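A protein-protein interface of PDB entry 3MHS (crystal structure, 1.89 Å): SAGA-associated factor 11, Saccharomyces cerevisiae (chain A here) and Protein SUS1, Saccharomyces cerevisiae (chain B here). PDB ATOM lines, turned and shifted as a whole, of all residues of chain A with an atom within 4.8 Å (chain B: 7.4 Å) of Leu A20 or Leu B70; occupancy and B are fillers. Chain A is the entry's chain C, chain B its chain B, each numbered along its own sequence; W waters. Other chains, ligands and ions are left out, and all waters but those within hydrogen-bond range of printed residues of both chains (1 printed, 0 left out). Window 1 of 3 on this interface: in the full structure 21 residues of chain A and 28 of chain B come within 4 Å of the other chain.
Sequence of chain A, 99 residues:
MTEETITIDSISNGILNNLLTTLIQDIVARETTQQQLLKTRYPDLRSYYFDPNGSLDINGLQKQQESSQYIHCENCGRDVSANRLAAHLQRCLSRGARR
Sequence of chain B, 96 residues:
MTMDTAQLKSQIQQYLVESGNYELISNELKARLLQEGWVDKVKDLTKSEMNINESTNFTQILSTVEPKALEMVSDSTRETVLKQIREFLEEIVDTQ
O of Asn A18 sits at hydrogen-bond distance from OG1 of Thr A21, at 3.4 Å.
The backbone NH (N) of Trp B38 lies within hydrogen-bond range of the backbone carbonyl oxygen (O) of Leu B33, at 2.9 Å.
O of Asn A17 is in hydrogen-bond range of OG1 of Thr A21, 2.9 Å away.
NE1 of Trp B38 is in hydrogen-bond range of O of Ala B69 (2.9 Å).
CD2 of Leu A16 touches NH1 of Arg B78 (3.6 Å).
Val B81 touches Leu A16 (CG1 to CD1, 3.8 Å).
Leu A19 touches Leu B29 (CB to CD2, 3.6 Å).
CD1 of Leu B33 touches CD2 of Leu A20, at 3.7 Å.
NH2 of Arg B78 touches CD1 of Leu A20 (3.8 Å).
CB of Thr A21 touches OE2 of Glu B66, at 3.4 Å.
Trp B38 touches Leu A23 (CZ3 to CD2, 3.5 Å).
Ile A24 touches Trp B38.
CD1 of Ile A24 touches CB of Ala B69, 3.6 Å away.
Leu B70 touches Ile A24.
Of the printed residues of chain B, Leu A20 touches Leu B33 (3.7 Å), Leu B70 (3.7 Å) and Arg B78 (3.8 Å).
Leu B70 touches two residues of chain A.
Printed residues of chain A within 4 Å of Leu B33: Leu A20 (3.7 Å) and Leu A23 (3.6 Å).
Of the printed residues of chain A, Ala B69 touches Ile A24.
Of the printed residues of chain A, Leu B29 touches Leu A19 (3.6 Å).
Asn A17 touches none of the printed residues of chain B.
The nearest residue of chain A that does not touch Leu B70 is Asn A17 (4.03 Å).
The nearest printed residue of chain B that does not touch Leu A19 is Val B81 (5.5 Å).
Of the 9 printed residues of chain A, 6 touch a printed residue of chain B.
Hydrophobic or aromatic side chains of chain A that line the printed part of chain B: Leu A16, Leu A19, Leu A20, Leu A23 and Ile A24.
Printed residues of chain B that touch a printed residue of chain A: Leu B29, Leu B33, Trp B38, Glu B66, Ala B69, Leu B70, Arg B78 and Val B81.
Hydrophobic or aromatic side chains of chain B that line the printed part of chain A: Leu B29, Leu B33, Trp B38, Ala B69, Leu B70 and Val B81.
Among the printed residues, no Asp or Glu carboxylate lies within 4 Å of a Lys or Arg side-chain nitrogen of the other chain.
Water W1 bridges ND2 of Asn A17 and NH2 of Arg B78.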
ATOM      1  N   LEU A  16      -7.060 -10.364  -5.239  1.00  0.00           N
ATOM      2  CA  LEU A  16      -7.833 -10.618  -4.022  1.00  0.00           C
ATOM      3  C   LEU A  16      -9.281 -10.210  -4.217  1.00  0.00           C
ATOM      4  O   LEU A  16     -10.187 -10.949  -3.847  1.00  0.00           O
ATOM      5  CB  LEU A  16      -7.239  -9.893  -2.813  1.00  0.00           C
ATOM      6  CG  LEU A  16      -7.960 -10.056  -1.465  1.00  0.00           C
ATOM      7  CD1 LEU A  16      -7.897 -11.492  -0.978  1.00  0.00           C
ATOM      8  CD2 LEU A  16      -7.401  -9.097  -0.395  1.00  0.00           C
ATOM      9  N   ASN A  17      -9.519  -9.055  -4.842  1.00  0.00           N
ATOM     10  CA  ASN A  17     -10.888  -8.660  -5.100  1.00  0.00           C
ATOM     11  C   ASN A  17     -11.585  -9.670  -6.035  1.00  0.00           C
ATOM     12  O   ASN A  17     -12.736 -10.022  -5.826  1.00  0.00           O
ATOM     13  CB  ASN A  17     -10.980  -7.217  -5.638  1.00  0.00           C
ATOM     14  CG  ASN A  17     -12.395  -6.700  -5.622  1.00  0.00           C
ATOM     15  OD1 ASN A  17     -13.060  -6.675  -6.650  1.00  0.00           O
ATOM     16  ND2 ASN A  17     -12.904  -6.413  -4.429  1.00  0.00           N
ATOM     17  N   ASN A  18     -10.890 -10.188  -7.039  1.00  0.00           N
ATOM     18  CA  ASN A  18     -11.514 -11.198  -7.890  1.00  0.00           C
ATOM     19  C   ASN A  18     -11.934 -12.452  -7.060  1.00  0.00           C
ATOM     20  O   ASN A  18     -13.066 -12.944  -7.138  1.00  0.00           O
ATOM     21  CB  ASN A  18     -10.581 -11.579  -9.040  1.00  0.00           C
ATOM     22  CG  ASN A  18     -10.703 -10.652 -10.226  1.00  0.00           C
ATOM     23  OD1 ASN A  18     -10.403 -11.025 -11.366  1.00  0.00           O
ATOM     24  ND2 ASN A  18     -11.170  -9.437  -9.967  1.00  0.00           N
ATOM     25  N   LEU A  19     -11.039 -12.890  -6.196  1.00  0.00           N
ATOM     26  CA  LEU A  19     -11.289 -14.092  -5.391  1.00  0.00           C
ATOM     27  C   LEU A  19     -12.422 -13.880  -4.407  1.00  0.00           C
ATOM     28  O   LEU A  19     -13.308 -14.720  -4.299  1.00  0.00           O
ATOM     29  CB  LEU A  19     -10.009 -14.479  -4.652  1.00  0.00           C
ATOM     30  CG  LEU A  19      -8.897 -15.053  -5.531  1.00  0.00           C
ATOM     31  CD1 LEU A  19      -7.581 -15.075  -4.779  1.00  0.00           C
ATOM     32  CD2 LEU A  19      -9.262 -16.490  -5.969  1.00  0.00           C
ATOM     33  N   LEU A  20     -12.420 -12.742  -3.717  1.00  0.00           N
ATOM     34  CA  LEU A  20     -13.429 -12.472  -2.697  1.00  0.00           C
ATOM     35  C   LEU A  20     -14.828 -12.264  -3.302  1.00  0.00           C
ATOM     36  O   LEU A  20     -15.794 -12.753  -2.760  1.00  0.00           O
ATOM     37  CB  LEU A  20     -13.057 -11.238  -1.859  1.00  0.00           C
ATOM     38  CG  LEU A  20     -11.897 -11.366  -0.870  1.00  0.00           C
ATOM     39  CD1 LEU A  20     -11.498  -9.940  -0.335  1.00  0.00           C
ATOM     40  CD2 LEU A  20     -12.244 -12.350   0.257  1.00  0.00           C
ATOM     41  N   THR A  21     -14.942 -11.508  -4.395  1.00  0.00           N
ATOM     42  CA  THR A  21     -16.268 -11.255  -4.982  1.00  0.00           C
ATOM     43  C   THR A  21     -16.887 -12.527  -5.594  1.00  0.00           C
ATOM     44  O   THR A  21     -18.092 -12.726  -5.530  1.00  0.00           O
ATOM     45  CB  THR A  21     -16.245 -10.121  -6.040  1.00  0.00           C
ATOM     46  OG1 THR A  21     -15.340 -10.455  -7.097  1.00  0.00           O
ATOM     47  CG2 THR A  21     -15.857  -8.780  -5.404  1.00  0.00           C
ATOM     48  N   THR A  22     -16.054 -13.385  -6.175  1.00  0.00           N
ATOM     49  CA  THR A  22     -16.498 -14.707  -6.642  1.00  0.00           C
ATOM     50  C   THR A  22     -17.075 -15.561  -5.522  1.00  0.00           C
ATOM     51  O   THR A  22     -18.150 -16.145  -5.677  1.00  0.00           O
ATOM     52  CB  THR A  22     -15.372 -15.491  -7.288  1.00  0.00           C
ATOM     53  OG1 THR A  22     -14.821 -14.737  -8.369  1.00  0.00           O
ATOM     54  CG2 THR A  22     -15.872 -16.828  -7.801  1.00  0.00           C
ATOM     55  N   LEU A  23     -16.341 -15.655  -4.415  1.00  0.00           N
ATOM     56  CA  LEU A  23     -16.789 -16.401  -3.263  1.00  0.00           C
ATOM     57  C   LEU A  23     -18.071 -15.827  -2.683  1.00  0.00           C
ATOM     58  O   LEU A  23     -18.989 -16.575  -2.369  1.00  0.00           O
ATOM     59  CB  LEU A  23     -15.687 -16.436  -2.196  1.00  0.00           C
ATOM     60  CG  LEU A  23     -15.941 -17.231  -0.917  1.00  0.00           C
ATOM     61  CD1 LEU A  23     -16.278 -18.701  -1.226  1.00  0.00           C
ATOM     62  CD2 LEU A  23     -14.695 -17.111   0.004  1.00  0.00           C
ATOM     63  N   ILE A  24     -18.138 -14.504  -2.560  1.00  0.00           N
ATOM     64  CA  ILE A  24     -19.313 -13.849  -2.025  1.00  0.00           C
ATOM     65  C   ILE A  24     -20.513 -14.180  -2.925  1.00  0.00           C
ATOM     66  O   ILE A  24     -21.570 -14.625  -2.456  1.00  0.00           O
ATOM     67  CB  ILE A  24     -19.102 -12.318  -1.957  1.00  0.00           C
ATOM     68  CG1 ILE A  24     -18.177 -11.965  -0.784  1.00  0.00           C
ATOM     69  CG2 ILE A  24     -20.439 -11.624  -1.823  1.00  0.00           C
ATOM     70  CD1 ILE A  24     -17.644 -10.522  -0.789  1.00  0.00           C
ATOM     71  N   LEU B  29      -6.994 -18.711   1.123  1.00  0.00           N
ATOM     72  CA  LEU B  29      -8.029 -17.684   1.381  1.00  0.00           C
ATOM     73  C   LEU B  29      -9.328 -18.329   1.890  1.00  0.00           C
ATOM     74  O   LEU B  29      -9.868 -17.924   2.918  1.00  0.00           O
ATOM     75  CB  LEU B  29      -8.349 -16.892   0.122  1.00  0.00           C
ATOM     76  CG  LEU B  29      -9.470 -15.857   0.206  1.00  0.00           C
ATOM     77  CD1 LEU B  29      -9.111 -14.751   1.240  1.00  0.00           C
ATOM     78  CD2 LEU B  29      -9.709 -15.257  -1.189  1.00  0.00           C
ATOM     79  N   LEU B  33     -10.954 -17.742   5.721  1.00  0.00           N
ATOM     80  CA  LEU B  33     -12.266 -17.147   5.881  1.00  0.00           C
ATOM     81  C   LEU B  33     -13.250 -18.088   6.553  1.00  0.00           C
ATOM     82  O   LEU B  33     -14.104 -17.662   7.340  1.00  0.00           O
ATOM     83  CB  LEU B  33     -12.809 -16.721   4.530  1.00  0.00           C
ATOM     84  CG  LEU B  33     -12.029 -15.605   3.824  1.00  0.00           C
ATOM     85  CD1 LEU B  33     -12.614 -15.366   2.388  1.00  0.00           C
ATOM     86  CD2 LEU B  33     -12.061 -14.320   4.630  1.00  0.00           C
ATOM     87  N   TRP B  38     -16.129 -16.083   8.751  1.00  0.00           N
ATOM     88  CA  TRP B  38     -16.632 -15.136   7.744  1.00  0.00           C
ATOM     89  C   TRP B  38     -17.652 -15.765   6.791  1.00  0.00           C
ATOM     90  O   TRP B  38     -18.624 -15.108   6.385  1.00  0.00           O
ATOM     91  CB  TRP B  38     -15.456 -14.551   6.959  1.00  0.00           C
ATOM     92  CG  TRP B  38     -15.795 -13.606   5.835  1.00  0.00           C
ATOM     93  CD1 TRP B  38     -15.885 -12.237   5.905  1.00  0.00           C
ATOM     94  CD2 TRP B  38     -16.035 -13.951   4.465  1.00  0.00           C
ATOM     95  NE1 TRP B  38     -16.179 -11.724   4.666  1.00  0.00           N
ATOM     96  CE2 TRP B  38     -16.248 -12.750   3.762  1.00  0.00           C
ATOM     97  CE3 TRP B  38     -16.071 -15.154   3.764  1.00  0.00           C
ATOM     98  CZ2 TRP B  38     -16.510 -12.724   2.397  1.00  0.00           C
ATOM     99  CZ3 TRP B  38     -16.329 -15.127   2.405  1.00  0.00           C
ATOM    100  CH2 TRP B  38     -16.553 -13.916   1.741  1.00  0.00           C
ATOM    101  N   VAL B  42     -21.467 -14.374   6.352  1.00  0.00           N
ATOM    102  CA  VAL B  42     -21.996 -13.881   5.073  1.00  0.00           C
ATOM    103  C   VAL B  42     -23.307 -14.550   4.712  1.00  0.00           C
ATOM    104  O   VAL B  42     -24.198 -13.935   4.106  1.00  0.00           O
ATOM    105  CB  VAL B  42     -21.001 -14.102   3.923  1.00  0.00           C
ATOM    106  CG1 VAL B  42     -21.650 -13.754   2.597  1.00  0.00           C
ATOM    107  CG2 VAL B  42     -19.761 -13.288   4.134  1.00  0.00           C
ATOM    108  N   LEU B  45     -25.810 -12.751   7.066  1.00  0.00           N
ATOM    109  CA  LEU B  45     -26.035 -11.432   6.477  1.00  0.00           C
ATOM    110  C   LEU B  45     -26.997 -11.544   5.302  1.00  0.00           C
ATOM    111  O   LEU B  45     -27.889 -10.720   5.167  1.00  0.00           O
ATOM    112  CB  LEU B  45     -24.702 -10.841   5.992  1.00  0.00           C
ATOM    113  CG  LEU B  45     -24.699  -9.540   5.178  1.00  0.00           C
ATOM    114  CD1 LEU B  45     -25.332  -8.373   5.925  1.00  0.00           C
ATOM    115  CD2 LEU B  45     -23.262  -9.199   4.757  1.00  0.00           C
ATOM    116  N   VAL B  65     -25.424  -7.133   0.137  1.00  0.00           N
ATOM    117  CA  VAL B  65     -24.547  -8.092   0.834  1.00  0.00           C
ATOM    118  C   VAL B  65     -23.070  -7.919   0.487  1.00  0.00           C
ATOM    119  O   VAL B  65     -22.219  -7.867   1.379  1.00  0.00           O
ATOM    120  CB  VAL B  65     -24.942  -9.541   0.550  1.00  0.00           C
ATOM    121  CG1 VAL B  65     -23.952 -10.513   1.241  1.00  0.00           C
ATOM    122  CG2 VAL B  65     -26.361  -9.786   1.014  1.00  0.00           C
ATOM    123  N   GLU B  66     -22.770  -7.806  -0.799  1.00  0.00           N
ATOM    124  CA  GLU B  66     -21.387  -7.836  -1.249  1.00  0.00           C
ATOM    125  C   GLU B  66     -20.509  -6.741  -0.653  1.00  0.00           C
ATOM    126  O   GLU B  66     -19.452  -7.040  -0.093  1.00  0.00           O
ATOM    127  CB  GLU B  66     -21.296  -7.825  -2.772  1.00  0.00           C
ATOM    128  CG  GLU B  66     -19.860  -7.912  -3.283  1.00  0.00           C
ATOM    129  CD  GLU B  66     -19.801  -8.285  -4.746  1.00  0.00           C
ATOM    130  OE1 GLU B  66     -20.061  -7.455  -5.602  1.00  0.00           O
ATOM    131  OE2 GLU B  66     -19.466  -9.417  -5.062  1.00  0.00           O
ATOM    132  N   PRO B  67     -20.940  -5.479  -0.739  1.00  0.00           N
ATOM    133  CA  PRO B  67     -20.080  -4.463  -0.158  1.00  0.00           C
ATOM    134  C   PRO B  67     -19.774  -4.747   1.299  1.00  0.00           C
ATOM    135  O   PRO B  67     -18.652  -4.557   1.747  1.00  0.00           O
ATOM    136  CB  PRO B  67     -20.920  -3.177  -0.281  1.00  0.00           C
ATOM    137  CG  PRO B  67     -21.864  -3.441  -1.412  1.00  0.00           C
ATOM    138  CD  PRO B  67     -22.172  -4.902  -1.318  1.00  0.00           C
ATOM    139  N   LYS B  68     -20.783  -5.178   2.041  1.00  0.00           N
ATOM    140  CA  LYS B  68     -20.634  -5.402   3.474  1.00  0.00           C
ATOM    141  C   LYS B  68     -19.717  -6.599   3.735  1.00  0.00           C
ATOM    142  O   LYS B  68     -18.812  -6.517   4.563  1.00  0.00           O
ATOM    143  CB  LYS B  68     -22.006  -5.617   4.121  1.00  0.00           C
ATOM    144  CG  LYS B  68     -21.975  -6.022   5.597  1.00  0.00           C
ATOM    145  CD  LYS B  68     -22.110  -4.849   6.555  1.00  0.00           C
ATOM    146  CE  LYS B  68     -20.794  -4.097   6.765  1.00  0.00           C
ATOM    147  NZ  LYS B  68     -19.674  -4.990   7.189  1.00  0.00           N
ATOM    148  N   ALA B  69     -19.942  -7.690   3.011  1.00  0.00           N
ATOM    149  CA  ALA B  69     -19.098  -8.898   3.121  1.00  0.00           C
ATOM    150  C   ALA B  69     -17.622  -8.598   2.854  1.00  0.00           C
ATOM    151  O   ALA B  69     -16.745  -9.150   3.503  1.00  0.00           O
ATOM    152  CB  ALA B  69     -19.594  -9.970   2.168  1.00  0.00           C
ATOM    153  N   LEU B  70     -17.348  -7.716   1.898  1.00  0.00           N
ATOM    154  CA  LEU B  70     -15.966  -7.292   1.616  1.00  0.00           C
ATOM    155  C   LEU B  70     -15.385  -6.514   2.803  1.00  0.00           C
ATOM    156  O   LEU B  70     -14.205  -6.657   3.125  1.00  0.00           O
ATOM    157  CB  LEU B  70     -15.899  -6.433   0.349  1.00  0.00           C
ATOM    158  CG  LEU B  70     -16.093  -7.074  -1.028  1.00  0.00           C
ATOM    159  CD1 LEU B  70     -16.183  -5.988  -2.130  1.00  0.00           C
ATOM    160  CD2 LEU B  70     -14.943  -8.056  -1.326  1.00  0.00           C
ATOM    161  N   GLU B  71     -16.200  -5.702   3.468  1.00  0.00           N
ATOM    162  CA  GLU B  71     -15.699  -4.925   4.606  1.00  0.00           C
ATOM    163  C   GLU B  71     -15.401  -5.870   5.767  1.00  0.00           C
ATOM    164  O   GLU B  71     -14.492  -5.614   6.557  1.00  0.00           O
ATOM    165  CB  GLU B  71     -16.699  -3.856   5.062  1.00  0.00           C
ATOM    166  CG  GLU B  71     -17.118  -2.841   4.001  1.00  0.00           C
ATOM    167  CD  GLU B  71     -18.292  -1.970   4.457  1.00  0.00           C
ATOM    168  OE1 GLU B  71     -19.056  -1.462   3.595  1.00  0.00           O
ATOM    169  OE2 GLU B  71     -18.456  -1.796   5.687  1.00  0.00           O
ATOM    170  N   MET B  72     -16.152  -6.973   5.841  1.00  0.00           N
ATOM    171  CA  MET B  72     -16.058  -7.931   6.964  1.00  0.00           C
ATOM    172  C   MET B  72     -14.786  -8.761   6.983  1.00  0.00           C
ATOM    173  O   MET B  72     -14.490  -9.416   7.978  1.00  0.00           O
ATOM    174  CB  MET B  72     -17.259  -8.885   6.970  1.00  0.00           C
ATOM    175  CG  MET B  72     -18.591  -8.202   7.284  1.00  0.00           C
ATOM    176  SD  MET B  72     -20.011  -9.199   6.802  1.00  0.00           S
ATOM    177  CE  MET B  72     -19.851 -10.628   7.859  1.00  0.00           C
ATOM    178  N   VAL B  73     -14.045  -8.762   5.886  1.00  0.00           N
ATOM    179  CA  VAL B  73     -12.783  -9.495   5.834  1.00  0.00           C
ATOM    180  C   VAL B  73     -11.804  -8.926   6.859  1.00  0.00           C
ATOM    181  O   VAL B  73     -11.504  -7.716   6.854  1.00  0.00           O
ATOM    182  CB  VAL B  73     -12.172  -9.467   4.414  1.00  0.00           C
ATOM    183  CG1 VAL B  73     -10.885 -10.285   4.362  1.00  0.00           C
ATOM    184  CG2 VAL B  73     -13.197 -10.011   3.400  1.00  0.00           C
ATOM    185  N   SER B  74     -11.338  -9.796   7.756  1.00  0.00           N
ATOM    186  CA  SER B  74     -10.409  -9.417   8.816  1.00  0.00           C
ATOM    187  C   SER B  74      -9.191  -8.783   8.189  1.00  0.00           C
ATOM    188  O   SER B  74      -8.829  -9.119   7.061  1.00  0.00           O
ATOM    189  CB  SER B  74      -9.968 -10.647   9.635  1.00  0.00           C
ATOM    190  OG  SER B  74      -9.199 -11.550   8.841  1.00  0.00           O
ATOM    191  N   THR B  77      -6.580 -11.559   7.638  1.00  0.00           N
ATOM    192  CA  THR B  77      -6.706 -12.357   6.420  1.00  0.00           C
ATOM    193  C   THR B  77      -6.305 -11.561   5.165  1.00  0.00           C
ATOM    194  O   THR B  77      -5.601 -12.068   4.295  1.00  0.00           O
ATOM    195  CB  THR B  77      -8.110 -12.964   6.304  1.00  0.00           C
ATOM    196  OG1 THR B  77      -8.230 -14.029   7.255  1.00  0.00           O
ATOM    197  CG2 THR B  77      -8.359 -13.512   4.919  1.00  0.00           C
ATOM    198  N   ARG B  78      -6.704 -10.295   5.102  1.00  0.00           N
ATOM    199  CA  ARG B  78      -6.408  -9.459   3.938  1.00  0.00           C
ATOM    200  C   ARG B  78      -4.896  -9.309   3.728  1.00  0.00           C
ATOM    201  O   ARG B  78      -4.382  -9.585   2.647  1.00  0.00           O
ATOM    202  CB  ARG B  78      -7.068  -8.081   4.086  1.00  0.00           C
ATOM    203  CG  ARG B  78      -6.550  -7.020   3.125  1.00  0.00           C
ATOM    204  CD  ARG B  78      -7.480  -5.804   3.066  1.00  0.00           C
ATOM    205  NE  ARG B  78      -8.783  -6.149   2.506  1.00  0.00           N
ATOM    206  CZ  ARG B  78      -9.078  -6.113   1.209  1.00  0.00           C
ATOM    207  NH1 ARG B  78      -8.172  -5.703   0.327  1.00  0.00           N
ATOM    208  NH2 ARG B  78     -10.288  -6.470   0.801  1.00  0.00           N
ATOM    209  N   VAL B  81      -2.928 -12.769   2.967  1.00  0.00           N
ATOM    210  CA  VAL B  81      -3.193 -13.265   1.618  1.00  0.00           C
ATOM    211  C   VAL B  81      -2.577 -12.352   0.559  1.00  0.00           C
ATOM    212  O   VAL B  81      -2.019 -12.845  -0.421  1.00  0.00           O
ATOM    213  CB  VAL B  81      -4.704 -13.511   1.397  1.00  0.00           C
ATOM    214  CG1 VAL B  81      -5.022 -13.792  -0.061  1.00  0.00           C
ATOM    215  CG2 VAL B  81      -5.141 -14.724   2.261  1.00  0.00           C
HETATM  216  O   HOH W   1     -11.460  -6.617  -2.121  1.00  0.00           O
